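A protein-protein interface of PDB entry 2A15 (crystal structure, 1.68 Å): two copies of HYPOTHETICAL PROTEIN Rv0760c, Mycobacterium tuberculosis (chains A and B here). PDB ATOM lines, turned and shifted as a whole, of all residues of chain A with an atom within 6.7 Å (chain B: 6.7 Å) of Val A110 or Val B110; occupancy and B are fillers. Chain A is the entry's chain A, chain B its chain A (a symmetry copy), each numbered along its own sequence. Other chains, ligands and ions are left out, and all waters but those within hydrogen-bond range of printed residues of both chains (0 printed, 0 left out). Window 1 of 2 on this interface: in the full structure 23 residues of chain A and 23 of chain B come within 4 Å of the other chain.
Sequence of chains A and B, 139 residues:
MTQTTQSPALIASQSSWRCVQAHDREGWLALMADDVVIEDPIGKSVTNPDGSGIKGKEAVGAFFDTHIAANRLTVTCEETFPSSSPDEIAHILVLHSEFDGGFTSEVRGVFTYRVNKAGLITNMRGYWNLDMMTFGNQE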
ATOM      1  N   ILE A  42      -5.323  13.043  19.546  1.00  0.00           N
ATOM      2  CA  ILE A  42      -6.650  13.634  19.556  1.00  0.00           C
ATOM      3  C   ILE A  42      -7.580  12.695  20.366  1.00  0.00           C
ATOM      4  O   ILE A  42      -7.547  11.468  20.173  1.00  0.00           O
ATOM      5  CB  ILE A  42      -7.191  13.700  18.120  1.00  0.00           C
ATOM      6  CG1 ILE A  42      -6.296  14.577  17.253  1.00  0.00           C
ATOM      7  CG2 ILE A  42      -8.628  14.230  18.134  1.00  0.00           C
ATOM      8  CD1 ILE A  42      -6.561  14.355  15.745  1.00  0.00           C
ATOM      9  N   PHE A  81       4.115  13.868   4.370  1.00  0.00           N
ATOM     10  CA  PHE A  81       3.061  14.224   3.414  1.00  0.00           C
ATOM     11  C   PHE A  81       2.796  15.736   3.447  1.00  0.00           C
ATOM     12  O   PHE A  81       1.998  16.265   4.212  1.00  0.00           O
ATOM     13  CB  PHE A  81       1.765  13.460   3.735  1.00  0.00           C
ATOM     14  CG  PHE A  81       1.894  11.970   3.573  1.00  0.00           C
ATOM     15  CD1 PHE A  81       1.632  11.372   2.346  1.00  0.00           C
ATOM     16  CD2 PHE A  81       2.303  11.162   4.649  1.00  0.00           C
ATOM     17  CE1 PHE A  81       1.724   9.999   2.177  1.00  0.00           C
ATOM     18  CE2 PHE A  81       2.384   9.771   4.491  1.00  0.00           C
ATOM     19  CZ  PHE A  81       2.087   9.201   3.255  1.00  0.00           C
ATOM     20  N   PRO A  82       3.503  16.479   2.561  1.00  0.00           N
ATOM     21  CA  PRO A  82       3.215  17.867   2.363  1.00  0.00           C
ATOM     22  C   PRO A  82       1.744  18.039   1.925  1.00  0.00           C
ATOM     23  O   PRO A  82       1.171  17.088   1.311  1.00  0.00           O
ATOM     24  CB  PRO A  82       4.132  18.221   1.168  1.00  0.00           C
ATOM     25  CG  PRO A  82       5.215  17.265   1.222  1.00  0.00           C
ATOM     26  CD  PRO A  82       4.574  15.988   1.672  1.00  0.00           C
ATOM     27  N   ALA A  90       1.598  16.751   7.254  1.00  0.00           N
ATOM     28  CA  ALA A  90       1.373  15.507   8.040  1.00  0.00           C
ATOM     29  C   ALA A  90       2.579  14.567   7.925  1.00  0.00           C
ATOM     30  O   ALA A  90       3.294  14.580   6.924  1.00  0.00           O
ATOM     31  CB  ALA A  90       0.107  14.810   7.529  1.00  0.00           C
ATOM     32  N   HIS A  91       2.782  13.702   8.919  1.00  0.00           N
ATOM     33  CA  HIS A  91       3.905  12.755   8.908  1.00  0.00           C
ATOM     34  C   HIS A  91       3.402  11.477   9.531  1.00  0.00           C
ATOM     35  O   HIS A  91       2.468  11.512  10.341  1.00  0.00           O
ATOM     36  CB  HIS A  91       5.050  13.257   9.784  1.00  0.00           C
ATOM     37  CG  HIS A  91       5.577  14.615   9.425  1.00  0.00           C
ATOM     38  ND1 HIS A  91       6.562  14.809   8.474  1.00  0.00           N
ATOM     39  CD2 HIS A  91       5.313  15.831   9.956  1.00  0.00           C
ATOM     40  CE1 HIS A  91       6.844  16.105   8.409  1.00  0.00           C
ATOM     41  NE2 HIS A  91       6.100  16.742   9.301  1.00  0.00           N
ATOM     42  N   ILE A  92       3.990  10.363   9.131  1.00  0.00           N
ATOM     43  CA  ILE A  92       3.871   9.134   9.908  1.00  0.00           C
ATOM     44  C   ILE A  92       5.082   9.133  10.830  1.00  0.00           C
ATOM     45  O   ILE A  92       6.239   9.162  10.371  1.00  0.00           O
ATOM     46  CB  ILE A  92       3.913   7.875   9.034  1.00  0.00           C
ATOM     47  CG1 ILE A  92       2.938   7.960   7.842  1.00  0.00           C
ATOM     48  CG2 ILE A  92       3.815   6.648   9.944  1.00  0.00           C
ATOM     49  CD1 ILE A  92       1.560   8.376   8.188  1.00  0.00           C
ATOM     50  N   LEU A  93       4.817   9.136  12.131  1.00  0.00           N
ATOM     51  CA  LEU A  93       5.898   9.090  13.127  1.00  0.00           C
ATOM     52  C   LEU A  93       5.804   7.820  13.957  1.00  0.00           C
ATOM     53  O   LEU A  93       4.703   7.307  14.239  1.00  0.00           O
ATOM     54  CB  LEU A  93       5.825  10.277  14.075  1.00  0.00           C
ATOM     55  CG  LEU A  93       5.747  11.700  13.523  1.00  0.00           C
ATOM     56  CD1 LEU A  93       5.704  12.702  14.667  1.00  0.00           C
ATOM     57  CD2 LEU A  93       6.943  11.911  12.604  1.00  0.00           C
ATOM     58  N   ARG A 108       2.866   3.887  16.326  1.00  0.00           N
ATOM     59  CA  ARG A 108       3.057   4.484  15.002  1.00  0.00           C
ATOM     60  C   ARG A 108       1.754   5.189  14.654  1.00  0.00           C
ATOM     61  O   ARG A 108       0.658   4.569  14.676  1.00  0.00           O
ATOM     62  CB  ARG A 108       3.370   3.370  14.016  1.00  0.00           C
ATOM     63  CG  ARG A 108       3.558   3.830  12.565  1.00  0.00           C
ATOM     64  CD  ARG A 108       4.238   2.698  11.779  1.00  0.00           C
ATOM     65  NE  ARG A 108       4.108   2.957  10.363  1.00  0.00           N
ATOM     66  CZ  ARG A 108       3.001   2.719   9.674  1.00  0.00           C
ATOM     67  NH1 ARG A 108       1.934   2.185  10.287  1.00  0.00           N
ATOM     68  NH2 ARG A 108       2.959   3.021   8.388  1.00  0.00           N
ATOM     69  N   GLY A 109       1.818   6.489  14.359  1.00  0.00           N
ATOM     70  CA  GLY A 109       0.566   7.265  14.161  1.00  0.00           C
ATOM     71  C   GLY A 109       0.783   8.329  13.101  1.00  0.00           C
ATOM     72  O   GLY A 109       1.929   8.537  12.667  1.00  0.00           O
ATOM     73  N   VAL A 110      -0.315   8.958  12.688  1.00  0.00           N
ATOM     74  CA  VAL A 110      -0.256  10.089  11.785  1.00  0.00           C
ATOM     75  C   VAL A 110      -0.246  11.322  12.677  1.00  0.00           C
ATOM     76  O   VAL A 110      -1.062  11.451  13.608  1.00  0.00           O
ATOM     77  CB  VAL A 110      -1.485  10.156  10.847  1.00  0.00           C
ATOM     78  CG1 VAL A 110      -1.648  11.574  10.242  1.00  0.00           C
ATOM     79  CG2 VAL A 110      -1.331   9.117   9.718  1.00  0.00           C
ATOM     80  N   PHE A 111       0.682  12.243  12.402  1.00  0.00           N
ATOM     81  CA  PHE A 111       0.689  13.506  13.139  1.00  0.00           C
ATOM     82  C   PHE A 111       0.575  14.675  12.161  1.00  0.00           C
ATOM     83  O   PHE A 111       1.308  14.714  11.166  1.00  0.00           O
ATOM     84  CB  PHE A 111       1.967  13.642  13.976  1.00  0.00           C
ATOM     85  CG  PHE A 111       2.013  12.640  15.112  1.00  0.00           C
ATOM     86  CD1 PHE A 111       1.754  13.030  16.420  1.00  0.00           C
ATOM     87  CD2 PHE A 111       2.274  11.309  14.820  1.00  0.00           C
ATOM     88  CE1 PHE A 111       1.786  12.047  17.436  1.00  0.00           C
ATOM     89  CE2 PHE A 111       2.292  10.345  15.836  1.00  0.00           C
ATOM     90  CZ  PHE A 111       2.042  10.740  17.106  1.00  0.00           C
ATOM     91  N   THR A 112      -0.345  15.577  12.452  1.00  0.00           N
ATOM     92  CA  THR A 112      -0.553  16.761  11.626  1.00  0.00           C
ATOM     93  C   THR A 112      -0.056  17.980  12.345  1.00  0.00           C
ATOM     94  O   THR A 112      -0.163  18.093  13.566  1.00  0.00           O
ATOM     95  CB  THR A 112      -2.039  16.976  11.197  1.00  0.00           C
ATOM     96  OG1 THR A 112      -2.887  17.254  12.327  1.00  0.00           O
ATOM     97  CG2 THR A 112      -2.555  15.713  10.433  1.00  0.00           C
ATOM     98  N   ARG A 125      -1.414  17.483  16.132  1.00  0.00           N
ATOM     99  CA  ARG A 125      -2.540  16.551  16.418  1.00  0.00           C
ATOM    100  C   ARG A 125      -2.118  15.155  16.004  1.00  0.00           C
ATOM    101  O   ARG A 125      -1.606  14.915  14.874  1.00  0.00           O
ATOM    102  CB  ARG A 125      -3.813  16.932  15.655  1.00  0.00           C
ATOM    103  CG  ARG A 125      -4.090  18.466  15.747  1.00  0.00           C
ATOM    104  CD  ARG A 125      -5.436  18.821  15.124  1.00  0.00           C
ATOM    105  NE  ARG A 125      -6.529  18.472  16.042  1.00  0.00           N
ATOM    106  CZ  ARG A 125      -7.599  17.760  15.699  1.00  0.00           C
ATOM    107  NH1 ARG A 125      -7.756  17.361  14.429  1.00  0.00           N
ATOM    108  NH2 ARG A 125      -8.550  17.508  16.615  1.00  0.00           N
ATOM    109  N   GLY A 126      -2.282  14.213  16.936  1.00  0.00           N
ATOM    110  CA  GLY A 126      -1.883  12.819  16.664  1.00  0.00           C
ATOM    111  C   GLY A 126      -3.047  11.818  16.553  1.00  0.00           C
ATOM    112  O   GLY A 126      -3.992  11.841  17.381  1.00  0.00           O
ATOM    113  N   TYR A 127      -2.968  10.959  15.536  1.00  0.00           N
ATOM    114  CA  TYR A 127      -3.976   9.910  15.286  1.00  0.00           C
ATOM    115  C   TYR A 127      -3.394   8.606  15.778  1.00  0.00           C
ATOM    116  O   TYR A 127      -2.754   7.844  15.046  1.00  0.00           O
ATOM    117  CB  TYR A 127      -4.357   9.845  13.782  1.00  0.00           C
ATOM    118  CG  TYR A 127      -5.074  11.079  13.361  1.00  0.00           C
ATOM    119  CD1 TYR A 127      -6.500  11.090  13.249  1.00  0.00           C
ATOM    120  CD2 TYR A 127      -4.352  12.270  13.005  1.00  0.00           C
ATOM    121  CE1 TYR A 127      -7.197  12.262  12.861  1.00  0.00           C
ATOM    122  CE2 TYR A 127      -5.057  13.435  12.593  1.00  0.00           C
ATOM    123  CZ  TYR A 127      -6.453  13.443  12.538  1.00  0.00           C
ATOM    124  OH  TYR A 127      -7.093  14.608  12.142  1.00  0.00           O
ATOM    125  N   TRP A 128      -3.612   8.374  17.086  1.00  0.00           N
ATOM    126  CA  TRP A 128      -3.312   7.074  17.683  1.00  0.00           C
ATOM    127  C   TRP A 128      -4.091   6.924  18.987  1.00  0.00           C
ATOM    128  O   TRP A 128      -4.725   7.861  19.472  1.00  0.00           O
ATOM    129  CB  TRP A 128      -1.806   6.888  17.941  1.00  0.00           C
ATOM    130  CG  TRP A 128      -1.212   7.909  18.915  1.00  0.00           C
ATOM    131  CD1 TRP A 128      -0.772   9.174  18.607  1.00  0.00           C
ATOM    132  CD2 TRP A 128      -0.974   7.733  20.330  1.00  0.00           C
ATOM    133  NE1 TRP A 128      -0.303   9.807  19.751  1.00  0.00           N
ATOM    134  CE2 TRP A 128      -0.398   8.937  20.812  1.00  0.00           C
ATOM    135  CE3 TRP A 128      -1.195   6.675  21.237  1.00  0.00           C
ATOM    136  CZ2 TRP A 128      -0.041   9.119  22.173  1.00  0.00           C
ATOM    137  CZ3 TRP A 128      -0.826   6.854  22.575  1.00  0.00           C
ATOM    138  CH2 TRP A 128      -0.257   8.059  23.027  1.00  0.00           C
ATOM    139  N   MET A 132      -3.286   0.895  20.072  1.00  0.00           N
ATOM    140  CA  MET A 132      -2.302   0.741  19.006  1.00  0.00           C
ATOM    141  C   MET A 132      -0.873   0.539  19.475  1.00  0.00           C
ATOM    142  O   MET A 132       0.003   0.178  18.691  1.00  0.00           O
ATOM    143  CB  MET A 132      -2.382   1.958  18.070  1.00  0.00           C
ATOM    144  CG  MET A 132      -3.768   2.077  17.460  1.00  0.00           C
ATOM    145  SD  MET A 132      -4.181   3.675  16.694  1.00  0.00           S
ATOM    146  CE  MET A 132      -2.870   3.898  15.513  1.00  0.00           C
ATOM    147  N   ILE B  42      -5.635  20.284   1.323  1.00  0.00           N
ATOM    148  CA  ILE B  42      -5.516  21.529   2.063  1.00  0.00           C
ATOM    149  C   ILE B  42      -4.589  22.473   1.255  1.00  0.00           C
ATOM    150  O   ILE B  42      -3.529  22.040   0.770  1.00  0.00           O
ATOM    151  CB  ILE B  42      -4.839  21.257   3.415  1.00  0.00           C
ATOM    152  CG1 ILE B  42      -5.680  20.297   4.248  1.00  0.00           C
ATOM    153  CG2 ILE B  42      -4.620  22.579   4.158  1.00  0.00           C
ATOM    154  CD1 ILE B  42      -4.868  19.688   5.417  1.00  0.00           C
ATOM    155  N   PHE B  81      -5.541   4.976  10.582  1.00  0.00           N
ATOM    156  CA  PHE B  81      -5.029   5.444  11.874  1.00  0.00           C
ATOM    157  C   PHE B  81      -6.162   6.056  12.708  1.00  0.00           C
ATOM    158  O   PHE B  81      -6.489   7.235  12.642  1.00  0.00           O
ATOM    159  CB  PHE B  81      -3.913   6.482  11.665  1.00  0.00           C
ATOM    160  CG  PHE B  81      -2.694   5.921  10.989  1.00  0.00           C
ATOM    161  CD1 PHE B  81      -1.670   5.360  11.742  1.00  0.00           C
ATOM    162  CD2 PHE B  81      -2.577   5.932   9.587  1.00  0.00           C
ATOM    163  CE1 PHE B  81      -0.525   4.855  11.143  1.00  0.00           C
ATOM    164  CE2 PHE B  81      -1.418   5.437   8.975  1.00  0.00           C
ATOM    165  CZ  PHE B  81      -0.397   4.908   9.761  1.00  0.00           C
ATOM    166  N   PRO B  82      -6.800   5.208  13.552  1.00  0.00           N
ATOM    167  CA  PRO B  82      -7.743   5.691  14.515  1.00  0.00           C
ATOM    168  C   PRO B  82      -7.063   6.720  15.443  1.00  0.00           C
ATOM    169  O   PRO B  82      -5.812   6.640  15.636  1.00  0.00           O
ATOM    170  CB  PRO B  82      -8.053   4.414  15.332  1.00  0.00           C
ATOM    171  CG  PRO B  82      -7.782   3.312  14.437  1.00  0.00           C
ATOM    172  CD  PRO B  82      -6.588   3.750  13.645  1.00  0.00           C
ATOM    173  N   ALA B  90      -7.727   9.240  10.618  1.00  0.00           N
ATOM    174  CA  ALA B  90      -6.866   9.515   9.436  1.00  0.00           C
ATOM    175  C   ALA B  90      -6.607   8.230   8.641  1.00  0.00           C
ATOM    176  O   ALA B  90      -6.608   7.133   9.200  1.00  0.00           O
ATOM    177  CB  ALA B  90      -5.539  10.121   9.910  1.00  0.00           C
ATOM    178  N   HIS B  91      -6.322   8.354   7.344  1.00  0.00           N
ATOM    179  CA  HIS B  91      -6.055   7.188   6.492  1.00  0.00           C
ATOM    180  C   HIS B  91      -4.982   7.601   5.516  1.00  0.00           C
ATOM    181  O   HIS B  91      -4.855   8.791   5.206  1.00  0.00           O
ATOM    182  CB  HIS B  91      -7.287   6.819   5.671  1.00  0.00           C
ATOM    183  CG  HIS B  91      -8.525   6.541   6.471  1.00  0.00           C
ATOM    184  ND1 HIS B  91      -8.817   5.294   6.992  1.00  0.00           N
ATOM    185  CD2 HIS B  91      -9.584   7.334   6.761  1.00  0.00           C
ATOM    186  CE1 HIS B  91      -9.990   5.353   7.610  1.00  0.00           C
ATOM    187  NE2 HIS B  91     -10.472   6.580   7.481  1.00  0.00           N
ATOM    188  N   ILE B  92      -4.201   6.634   5.065  1.00  0.00           N
ATOM    189  CA  ILE B  92      -3.397   6.821   3.863  1.00  0.00           C
ATOM    190  C   ILE B  92      -4.262   6.296   2.726  1.00  0.00           C
ATOM    191  O   ILE B  92      -4.662   5.117   2.715  1.00  0.00           O
ATOM    192  CB  ILE B  92      -2.086   6.026   3.898  1.00  0.00           C
ATOM    193  CG1 ILE B  92      -1.308   6.240   5.212  1.00  0.00           C
ATOM    194  CG2 ILE B  92      -1.338   6.264   2.584  1.00  0.00           C
ATOM    195  CD1 ILE B  92      -1.134   7.654   5.613  1.00  0.00           C
ATOM    196  N   LEU B  93      -4.580   7.179   1.787  1.00  0.00           N
ATOM    197  CA  LEU B  93      -5.372   6.787   0.613  1.00  0.00           C
ATOM    198  C   LEU B  93      -4.563   6.971  -0.663  1.00  0.00           C
ATOM    199  O   LEU B  93      -3.731   7.893  -0.777  1.00  0.00           O
ATOM    200  CB  LEU B  93      -6.634   7.628   0.492  1.00  0.00           C
ATOM    201  CG  LEU B  93      -7.582   7.766   1.683  1.00  0.00           C
ATOM    202  CD1 LEU B  93      -8.772   8.636   1.303  1.00  0.00           C
ATOM    203  CD2 LEU B  93      -7.997   6.367   2.116  1.00  0.00           C
ATOM    204  N   ARG B 108      -0.776   9.615  -3.558  1.00  0.00           N
ATOM    205  CA  ARG B 108      -0.910   8.930  -2.269  1.00  0.00           C
ATOM    206  C   ARG B 108      -0.776  10.001  -1.196  1.00  0.00           C
ATOM    207  O   ARG B 108       0.229  10.759  -1.162  1.00  0.00           O
ATOM    208  CB  ARG B 108       0.194   7.890  -2.164  1.00  0.00           C
ATOM    209  CG  ARG B 108       0.217   7.110  -0.843  1.00  0.00           C
ATOM    210  CD  ARG B 108       1.100   5.867  -1.028  1.00  0.00           C
ATOM    211  NE  ARG B 108       1.423   5.315   0.268  1.00  0.00           N
ATOM    212  CZ  ARG B 108       2.357   5.814   1.064  1.00  0.00           C
ATOM    213  NH1 ARG B 108       3.080   6.871   0.664  1.00  0.00           N
ATOM    214  NH2 ARG B 108       2.561   5.267   2.250  1.00  0.00           N
ATOM    215  N   GLY B 109      -1.775  10.123  -0.319  1.00  0.00           N
ATOM    216  CA  GLY B 109      -1.773  11.246   0.654  1.00  0.00           C
ATOM    217  C   GLY B 109      -2.391  10.792   1.963  1.00  0.00           C
ATOM    218  O   GLY B 109      -2.943   9.679   2.028  1.00  0.00           O
ATOM    219  N   VAL B 110      -2.266  11.641   2.980  1.00  0.00           N
ATOM    220  CA  VAL B 110      -2.920  11.414   4.253  1.00  0.00           C
ATOM    221  C   VAL B 110      -4.238  12.169   4.173  1.00  0.00           C
ATOM    222  O   VAL B 110      -4.284  13.349   3.777  1.00  0.00           O
ATOM    223  CB  VAL B 110      -2.096  11.962   5.442  1.00  0.00           C
ATOM    224  CG1 VAL B 110      -2.984  12.141   6.700  1.00  0.00           C
ATOM    225  CG2 VAL B 110      -0.933  10.999   5.752  1.00  0.00           C
ATOM    226  N   PHE B 111      -5.329  11.496   4.550  1.00  0.00           N
ATOM    227  CA  PHE B 111      -6.620  12.182   4.608  1.00  0.00           C
ATOM    228  C   PHE B 111      -7.200  12.069   6.018  1.00  0.00           C
ATOM    229  O   PHE B 111      -7.234  10.967   6.579  1.00  0.00           O
ATOM    230  CB  PHE B 111      -7.598  11.593   3.587  1.00  0.00           C
ATOM    231  CG  PHE B 111      -7.177  11.885   2.161  1.00  0.00           C
ATOM    232  CD1 PHE B 111      -7.820  12.863   1.411  1.00  0.00           C
ATOM    233  CD2 PHE B 111      -6.104  11.188   1.624  1.00  0.00           C
ATOM    234  CE1 PHE B 111      -7.367  13.110   0.095  1.00  0.00           C
ATOM    235  CE2 PHE B 111      -5.661  11.451   0.322  1.00  0.00           C
ATOM    236  CZ  PHE B 111      -6.298  12.404  -0.398  1.00  0.00           C
ATOM    237  N   THR B 112      -7.617  13.200   6.558  1.00  0.00           N
ATOM    238  CA  THR B 112      -8.218  13.245   7.886  1.00  0.00           C
ATOM    239  C   THR B 112      -9.691  13.508   7.773  1.00  0.00           C
ATOM    240  O   THR B 112     -10.146  14.248   6.900  1.00  0.00           O
ATOM    241  CB  THR B 112      -7.570  14.302   8.835  1.00  0.00           C
ATOM    242  OG1 THR B 112      -7.789  15.645   8.368  1.00  0.00           O
ATOM    243  CG2 THR B 112      -6.037  14.020   8.968  1.00  0.00           C
ATOM    244  N   ARG B 125      -9.932  16.434   4.979  1.00  0.00           N
ATOM    245  CA  ARG B 125      -8.745  17.274   4.655  1.00  0.00           C
ATOM    246  C   ARG B 125      -7.650  16.367   4.128  1.00  0.00           C
ATOM    247  O   ARG B 125      -7.308  15.308   4.728  1.00  0.00           O
ATOM    248  CB  ARG B 125      -8.217  18.027   5.882  1.00  0.00           C
ATOM    249  CG  ARG B 125      -9.384  18.686   6.685  1.00  0.00           C
ATOM    250  CD  ARG B 125      -8.850  19.563   7.812  1.00  0.00           C
ATOM    251  NE  ARG B 125      -8.369  20.844   7.274  1.00  0.00           N
ATOM    252  CZ  ARG B 125      -7.178  21.371   7.542  1.00  0.00           C
ATOM    253  NH1 ARG B 125      -6.351  20.751   8.396  1.00  0.00           N
ATOM    254  NH2 ARG B 125      -6.842  22.558   7.008  1.00  0.00           N
ATOM    255  N   GLY B 126      -7.115  16.742   2.964  1.00  0.00           N
ATOM    256  CA  GLY B 126      -6.059  15.927   2.334  1.00  0.00           C
ATOM    257  C   GLY B 126      -4.665  16.577   2.301  1.00  0.00           C
ATOM    258  O   GLY B 126      -4.528  17.783   1.975  1.00  0.00           O
ATOM    259  N   TYR B 127      -3.652  15.778   2.640  1.00  0.00           N
ATOM    260  CA  TYR B 127      -2.243  16.217   2.641  1.00  0.00           C
ATOM    261  C   TYR B 127      -1.602  15.663   1.391  1.00  0.00           C
ATOM    262  O   TYR B 127      -1.023  14.573   1.365  1.00  0.00           O
ATOM    263  CB  TYR B 127      -1.510  15.747   3.926  1.00  0.00           C
ATOM    264  CG  TYR B 127      -2.054  16.429   5.131  1.00  0.00           C
ATOM    265  CD1 TYR B 127      -1.371  17.547   5.704  1.00  0.00           C
ATOM    266  CD2 TYR B 127      -3.246  15.952   5.778  1.00  0.00           C
ATOM    267  CE1 TYR B 127      -1.886  18.216   6.844  1.00  0.00           C
ATOM    268  CE2 TYR B 127      -3.741  16.612   6.936  1.00  0.00           C
ATOM    269  CZ  TYR B 127      -3.090  17.734   7.453  1.00  0.00           C
ATOM    270  OH  TYR B 127      -3.620  18.350   8.577  1.00  0.00           O
ATOM    271  N   TRP B 128      -1.751  16.454   0.310  1.00  0.00           N
ATOM    272  CA  TRP B 128      -1.020  16.187  -0.927  1.00  0.00           C
ATOM    273  C   TRP B 128      -0.978  17.456  -1.774  1.00  0.00           C
ATOM    274  O   TRP B 128      -1.621  18.459  -1.466  1.00  0.00           O
ATOM    275  CB  TRP B 128      -1.645  15.033  -1.732  1.00  0.00           C
ATOM    276  CG  TRP B 128      -3.085  15.297  -2.181  1.00  0.00           C
ATOM    277  CD1 TRP B 128      -4.224  15.094  -1.440  1.00  0.00           C
ATOM    278  CD2 TRP B 128      -3.525  15.780  -3.471  1.00  0.00           C
ATOM    279  NE1 TRP B 128      -5.344  15.450  -2.179  1.00  0.00           N
ATOM    280  CE2 TRP B 128      -4.941  15.854  -3.431  1.00  0.00           C
ATOM    281  CE3 TRP B 128      -2.858  16.161  -4.655  1.00  0.00           C
ATOM    282  CZ2 TRP B 128      -5.712  16.300  -4.535  1.00  0.00           C
ATOM    283  CZ3 TRP B 128      -3.624  16.585  -5.746  1.00  0.00           C
ATOM    284  CH2 TRP B 128      -5.028  16.649  -5.679  1.00  0.00           C
ATOM    285  N   MET B 132       3.247  15.841  -5.983  1.00  0.00           N
ATOM    286  CA  MET B 132       3.280  14.448  -5.548  1.00  0.00           C
ATOM    287  C   MET B 132       2.634  13.461  -6.503  1.00  0.00           C
ATOM    288  O   MET B 132       2.792  12.250  -6.362  1.00  0.00           O
ATOM    289  CB  MET B 132       2.631  14.340  -4.159  1.00  0.00           C
ATOM    290  CG  MET B 132       3.373  15.199  -3.150  1.00  0.00           C
ATOM    291  SD  MET B 132       2.506  15.546  -1.589  1.00  0.00           S
ATOM    292  CE  MET B 132       2.119  13.920  -0.981  1.00  0.00           C
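Of the 17 printed residues of chain A, 11 touch a printed residue of chain B.
Among the printed residues, merely in contact across the chains: Phe A81 with Arg B108 (3.6 Å), Phe A81 with Gly B109 (3.8 Å), Phe A81 with Val B110 (3.4 Å), Phe A81 with Tyr B127 (3.6 Å), Ala A90 with Tyr B127 (3.4 Å), Ile A92 with Ile B92 (3.8 Å), Arg A108 with Phe B81 (3.6 Å), Gly A109 with Phe B81 (3.8 Å), Val A110 with Phe B81 (3.4 Å), Val A110 with Val B110 (3.8 Å), Thr A112 with Tyr B127 (3.4 Å), Tyr A127 with Phe B81 (3.6 Å), Tyr A127 with Ala B90 (3.4 Å) and Tyr A127 with Thr B112 (3.4 Å).
Of chain A, only Phe A81 and Val A110 come within 4 Å of Val B110.
Of the printed residues of chain A, Ile B92 touches Ile A92 (3.8 Å).
Of the printed residues of chain A, Pro B82 touches Tyr A127, Trp A128 and Met A132.
Printed residues of chain A within 4 Å of Tyr B127: Phe A81, Pro A82, Ala A90 and Thr A112.
Of the printed residues of chain A, Arg B108 touches Phe A81.
His B91 touches none of the printed residues of chain A.
The nearest residue of chain B that does not touch Val A110 is Ala B90 (4.2 Å).
The nearest residue of chain A that does not touch Val B110 is Ala A90 (4.2 Å).
The backbone carbonyl oxygen (O) of Pro A82 sits close to the side-chain sulfur (SD) of Met B132 (3.5 Å).
The backbone carbonyl oxygen (O) of Tyr A127 lies close to the backbone carbonyl oxygen (O) of Pro B82 (3.3 Å).
The side-chain sulfur (SD) of Met A132 lies close to the backbone carbonyl oxygen (O) of Pro B82 (3.5 Å).
The backbone NH (N) of Trp B128 lies within hydrogen-bond range of the backbone carbonyl oxygen (O) of Pro A82 (3.2 Å).
The backbone carbonyl oxygen of Pro A82 lies close to the backbone carbonyl oxygen of Tyr B127.
The backbone carbonyl oxygen (O) of Pro B82 is in hydrogen-bond range of the backbone NH (N) of Trp A128 (3.2 Å).
Phe A81 touches Arg B108, and with the chains exchanged Arg A108 touches Phe B81.
Phe A81 touches Val B110, and with the chains exchanged Val A110 touches Phe B81.
Pro A82 touches Met B132, and with the chains exchanged Met A132 touches Pro B82.
Val B110 touches its own counterpart, Val A110.
Of the 20 pairs that touch across the chains among the printed residues, 20 have their exchanged pair printed and touching as well.
N of Tyr B127 sits at hydrogen-bond distance from O of Val B110.
The backbone NH (N) of Phe A81 is in hydrogen-bond range of the backbone carbonyl oxygen (O) of Ala A90, at 2.8 Å.
The backbone NH (N) of Leu A93 sits at hydrogen-bond distance from the backbone carbonyl oxygen (O) of Gly A109 (3.0 Å).
The backbone NH (N) of Leu B93 sits at hydrogen-bond distance from the backbone carbonyl oxygen (O) of Gly B109.
The backbone NH (N) of Thr B112 sits at hydrogen-bond distance from the backbone carbonyl oxygen (O) of Arg B125 (2.8 Å).
The backbone NH of Thr A112 lies within hydrogen-bond range of the backbone carbonyl oxygen of Arg A125 (2.8 Å).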
